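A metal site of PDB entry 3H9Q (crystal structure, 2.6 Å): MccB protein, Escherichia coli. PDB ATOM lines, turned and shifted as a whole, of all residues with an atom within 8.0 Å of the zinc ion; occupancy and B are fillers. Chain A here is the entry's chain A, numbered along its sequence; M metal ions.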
ATOM      1  N   ASN A 227      10.532  26.329  23.100  1.00  0.00           N
ATOM      2  CA  ASN A 227      10.148  24.945  22.896  1.00  0.00           C
ATOM      3  C   ASN A 227       8.703  24.898  22.380  1.00  0.00           C
ATOM      4  O   ASN A 227       8.447  24.472  21.245  1.00  0.00           O
ATOM      5  CB  ASN A 227      10.239  24.189  24.224  1.00  0.00           C
ATOM      6  CG  ASN A 227      10.008  22.696  24.051  1.00  0.00           C
ATOM      7  OD1 ASN A 227       9.339  22.064  24.868  1.00  0.00           O
ATOM      8  ND2 ASN A 227      10.579  22.129  23.003  1.00  0.00           N
ATOM      9  N   VAL A 231       7.578  23.591  18.716  1.00  0.00           N
ATOM     10  CA  VAL A 231       6.889  22.323  18.532  1.00  0.00           C
ATOM     11  C   VAL A 231       5.770  22.499  17.515  1.00  0.00           C
ATOM     12  O   VAL A 231       5.553  21.627  16.683  1.00  0.00           O
ATOM     13  CB  VAL A 231       6.284  21.796  19.849  1.00  0.00           C
ATOM     14  CG1 VAL A 231       5.269  20.715  19.539  1.00  0.00           C
ATOM     15  CG2 VAL A 231       7.383  21.249  20.752  1.00  0.00           C
ATOM     16  N   TYR A 253      16.320  19.808  19.451  1.00  0.00           N
ATOM     17  CA  TYR A 253      14.957  19.431  19.088  1.00  0.00           C
ATOM     18  C   TYR A 253      14.768  19.304  17.581  1.00  0.00           C
ATOM     19  O   TYR A 253      15.132  20.205  16.822  1.00  0.00           O
ATOM     20  CB  TYR A 253      13.940  20.441  19.619  1.00  0.00           C
ATOM     21  CG  TYR A 253      12.511  20.131  19.194  1.00  0.00           C
ATOM     22  CD1 TYR A 253      11.798  19.093  19.794  1.00  0.00           C
ATOM     23  CD2 TYR A 253      11.904  20.835  18.155  1.00  0.00           C
ATOM     24  CE1 TYR A 253      10.519  18.750  19.363  1.00  0.00           C
ATOM     25  CE2 TYR A 253      10.613  20.489  17.709  1.00  0.00           C
ATOM     26  CZ  TYR A 253       9.941  19.441  18.318  1.00  0.00           C
ATOM     27  OH  TYR A 253       8.705  19.056  17.849  1.00  0.00           O
ATOM     28  N   THR A 258      12.283  13.638  17.539  1.00  0.00           N
ATOM     29  CA  THR A 258      12.947  13.835  18.822  1.00  0.00           C
ATOM     30  C   THR A 258      12.052  14.271  19.992  1.00  0.00           C
ATOM     31  O   THR A 258      10.920  14.718  19.781  1.00  0.00           O
ATOM     32  CB  THR A 258      14.092  14.871  18.668  1.00  0.00           C
ATOM     33  OG1 THR A 258      15.314  14.323  19.179  1.00  0.00           O
ATOM     34  CG2 THR A 258      13.772  16.166  19.405  1.00  0.00           C
ATOM     35  N   GLY A 259      12.573  14.157  21.203  1.00  0.00           N
ATOM     36  CA  GLY A 259      11.816  14.579  22.373  1.00  0.00           C
ATOM     37  C   GLY A 259      11.971  16.083  22.564  1.00  0.00           C
ATOM     38  O   GLY A 259      12.998  16.645  22.182  1.00  0.00           O
ATOM     39  N   CYS A 260      10.953  16.732  23.127  1.00  0.00           N
ATOM     40  CA  CYS A 260      10.986  18.186  23.365  1.00  0.00           C
ATOM     41  C   CYS A 260      11.430  18.417  24.793  1.00  0.00           C
ATOM     42  O   CYS A 260      11.551  17.465  25.565  1.00  0.00           O
ATOM     43  CB  CYS A 260       9.608  18.823  23.131  1.00  0.00           C
ATOM     44  SG  CYS A 260       8.434  18.549  24.466  1.00  0.00           S
ATOM     45  N   TYR A 261      11.653  19.691  25.145  1.00  0.00           N
ATOM     46  CA  TYR A 261      12.124  20.089  26.476  1.00  0.00           C
ATOM     47  C   TYR A 261      11.252  19.680  27.659  1.00  0.00           C
ATOM     48  O   TYR A 261      11.767  19.274  28.707  1.00  0.00           O
ATOM     49  CB  TYR A 261      12.333  21.618  26.497  1.00  0.00           C
ATOM     50  CG  TYR A 261      13.284  22.128  27.571  1.00  0.00           C
ATOM     51  CD1 TYR A 261      14.666  22.087  27.383  1.00  0.00           C
ATOM     52  CD2 TYR A 261      12.778  22.674  28.761  1.00  0.00           C
ATOM     53  CE1 TYR A 261      15.538  22.586  28.365  1.00  0.00           C
ATOM     54  CE2 TYR A 261      13.637  23.176  29.740  1.00  0.00           C
ATOM     55  CZ  TYR A 261      15.024  23.139  29.536  1.00  0.00           C
ATOM     56  OH  TYR A 261      15.870  23.661  30.496  1.00  0.00           O
ATOM     57  N   GLU A 262       9.930  19.785  27.504  1.00  0.00           N
ATOM     58  CA  GLU A 262       8.976  19.485  28.580  1.00  0.00           C
ATOM     59  C   GLU A 262       8.643  18.005  28.818  1.00  0.00           C
ATOM     60  O   GLU A 262       8.167  17.639  29.890  1.00  0.00           O
ATOM     61  CB  GLU A 262       7.679  20.268  28.352  1.00  0.00           C
ATOM     62  N   CYS A 263       8.889  17.172  27.814  1.00  0.00           N
ATOM     63  CA  CYS A 263       8.595  15.746  27.914  1.00  0.00           C
ATOM     64  C   CYS A 263       8.916  15.066  29.236  1.00  0.00           C
ATOM     65  O   CYS A 263       8.018  14.601  29.933  1.00  0.00           O
ATOM     66  CB  CYS A 263       9.309  14.994  26.790  1.00  0.00           C
ATOM     67  SG  CYS A 263       8.432  15.071  25.245  1.00  0.00           S
ATOM     68  N   GLN A 264      10.212  14.998  29.567  1.00  0.00           N
ATOM     69  CA  GLN A 264      10.671  14.350  30.782  1.00  0.00           C
ATOM     70  C   GLN A 264      10.644  15.241  32.029  1.00  0.00           C
ATOM     71  O   GLN A 264      11.514  15.145  32.892  1.00  0.00           O
ATOM     72  CB  GLN A 264      12.087  13.816  30.559  1.00  0.00           C
ATOM     73  CG  GLN A 264      12.280  13.028  29.261  1.00  0.00           C
ATOM     74  CD  GLN A 264      11.533  11.711  29.240  1.00  0.00           C
ATOM     75  OE1 GLN A 264      11.648  10.901  30.158  1.00  0.00           O
ATOM     76  NE2 GLN A 264      10.786  11.470  28.163  1.00  0.00           N
ATOM     77  N   MET A 340      15.893  12.948  27.496  1.00  0.00           N
ATOM     78  CA  MET A 340      14.839  13.835  26.983  1.00  0.00           C
ATOM     79  C   MET A 340      14.301  13.256  25.680  1.00  0.00           C
ATOM     80  O   MET A 340      14.131  13.964  24.692  1.00  0.00           O
ATOM     81  CB  MET A 340      15.371  15.247  26.722  1.00  0.00           C
ATOM     82  CG  MET A 340      15.807  15.984  27.964  1.00  0.00           C
ATOM     83  SD  MET A 340      15.936  17.768  27.680  1.00  0.00           S
ATOM     84  CE  MET A 340      15.940  18.379  29.349  1.00  0.00           C
ATOM     85  N   GLY A 341      14.030  11.951  25.681  1.00  0.00           N
ATOM     86  CA  GLY A 341      13.499  11.304  24.495  1.00  0.00           C
ATOM     87  C   GLY A 341      12.008  11.542  24.406  1.00  0.00           C
ATOM     88  O   GLY A 341      11.385  11.910  25.398  1.00  0.00           O
ATOM     89  N   ARG A 342      11.439  11.322  23.232  1.00  0.00           N
ATOM     90  CA  ARG A 342      10.007  11.520  23.043  1.00  0.00           C
ATOM     91  C   ARG A 342       9.183  10.690  24.019  1.00  0.00           C
ATOM     92  O   ARG A 342       9.480   9.531  24.305  1.00  0.00           O
ATOM     93  CB  ARG A 342       9.599  11.198  21.591  1.00  0.00           C
ATOM     94  N   SER A 343       8.135  11.333  24.542  1.00  0.00           N
ATOM     95  CA  SER A 343       7.197  10.730  25.478  1.00  0.00           C
ATOM     96  C   SER A 343       5.824  10.879  24.865  1.00  0.00           C
ATOM     97  O   SER A 343       5.441  11.971  24.428  1.00  0.00           O
ATOM     98  CB  SER A 343       7.256  11.462  26.825  1.00  0.00           C
ATOM     99  OG  SER A 343       6.036  11.293  27.551  1.00  0.00           O
ATOM    100  N   PRO A 344       5.045   9.786  24.808  1.00  0.00           N
ATOM    101  CA  PRO A 344       3.707   9.885  24.215  1.00  0.00           C
ATOM    102  C   PRO A 344       2.846  10.750  25.130  1.00  0.00           C
ATOM    103  O   PRO A 344       1.991  11.518  24.665  1.00  0.00           O
ATOM    104  CB  PRO A 344       3.224   8.431  24.196  1.00  0.00           C
ATOM    105  CG  PRO A 344       4.508   7.634  24.187  1.00  0.00           C
ATOM    106  CD  PRO A 344       5.363   8.389  25.167  1.00  0.00           C
ATOM    107  N   VAL A 345       3.110  10.613  26.422  1.00  0.00           N
ATOM    108  CA  VAL A 345       2.413  11.340  27.475  1.00  0.00           C
ATOM    109  C   VAL A 345       2.966  12.765  27.672  1.00  0.00           C
ATOM    110  O   VAL A 345       3.306  13.154  28.788  1.00  0.00           O
ATOM    111  CB  VAL A 345       2.535  10.585  28.830  1.00  0.00           C
ATOM    112  CG1 VAL A 345       1.460  11.032  29.792  1.00  0.00           C
ATOM    113  CG2 VAL A 345       2.458   9.080  28.594  1.00  0.00           C
ATOM    114  N   CYS A 346       3.041  13.554  26.592  1.00  0.00           N
ATOM    115  CA  CYS A 346       3.559  14.908  26.701  1.00  0.00           C
ATOM    116  C   CYS A 346       2.489  15.968  26.538  1.00  0.00           C
ATOM    117  O   CYS A 346       1.661  15.895  25.632  1.00  0.00           O
ATOM    118  CB  CYS A 346       4.663  15.162  25.671  1.00  0.00           C
ATOM    119  SG  CYS A 346       5.359  16.840  25.724  1.00  0.00           S
ATOM    120  N   SER A 347       2.515  16.961  27.416  1.00  0.00           N
ATOM    121  CA  SER A 347       1.528  18.037  27.389  1.00  0.00           C
ATOM    122  C   SER A 347       1.838  19.115  26.354  1.00  0.00           C
ATOM    123  O   SER A 347       1.065  20.068  26.213  1.00  0.00           O
ATOM    124  CB  SER A 347       1.410  18.641  28.773  1.00  0.00           C
ATOM    125  N   VAL A 348       2.950  18.980  25.629  1.00  0.00           N
ATOM    126  CA  VAL A 348       3.337  19.976  24.625  1.00  0.00           C
ATOM    127  C   VAL A 348       3.266  19.425  23.210  1.00  0.00           C
ATOM    128  O   VAL A 348       2.867  20.136  22.279  1.00  0.00           O
ATOM    129  CB  VAL A 348       4.776  20.521  24.881  1.00  0.00           C
ATOM    130  CG1 VAL A 348       5.105  21.597  23.857  1.00  0.00           C
ATOM    131  CG2 VAL A 348       4.877  21.090  26.284  1.00  0.00           C
ATOM    132  N   CYS A 349       3.660  18.174  23.025  1.00  0.00           N
ATOM    133  CA  CYS A 349       3.603  17.553  21.699  1.00  0.00           C
ATOM    134  C   CYS A 349       3.188  16.084  21.757  1.00  0.00           C
ATOM    135  O   CYS A 349       3.560  15.303  20.877  1.00  0.00           O
ATOM    136  CB  CYS A 349       4.957  17.682  20.992  1.00  0.00           C
ATOM    137  SG  CYS A 349       6.302  16.662  21.648  1.00  0.00           S
ATOM    138  N   GLY A 350       2.431  15.718  22.786  1.00  0.00           N
ATOM    139  CA  GLY A 350       1.982  14.341  22.955  1.00  0.00           C
ATOM    140  C   GLY A 350       0.716  13.932  22.212  1.00  0.00           C
ATOM    141  O   GLY A 350       0.347  14.546  21.212  1.00  0.00           O
ATOM    142  N   ASN A 351       0.060  12.883  22.722  1.00  0.00           N
ATOM    143  CA  ASN A 351      -1.172  12.344  22.136  1.00  0.00           C
ATOM    144  C   ASN A 351      -2.214  13.418  21.837  1.00  0.00           C
ATOM    145  O   ASN A 351      -2.501  13.636  20.637  1.00  0.00           O
ATOM    146  CB  ASN A 351      -1.772  11.292  23.069  1.00  0.00           C
HETATM  147 ZN    ZN M   1       7.061  16.431  23.929  1.00  0.00          ZN
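The side-chain amide oxygen (OD1) of Asn 227 lies close to the side-chain sulfur (SG) of Cys 260.
The side-chain sulfur (SG) of Cys 346 sits close to the backbone NH (N) of Val 348 (3.2 Å).
N of Glu 262 lies close to SG of Cys 260 (3.6 Å).
The nearest printed residue that does not touch the zinc ion is Ser 343 (4.8 Å).
The zinc ion is bound by the side-chain sulfur (SG) of Cys 263 (2.3 Å), the side-chain sulfur (SG) of Cys 349 (2.4 Å), the side-chain sulfur (SG) of Cys 346 (2.5 Å) and the side-chain sulfur (SG) of Cys 260 (2.6 Å).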
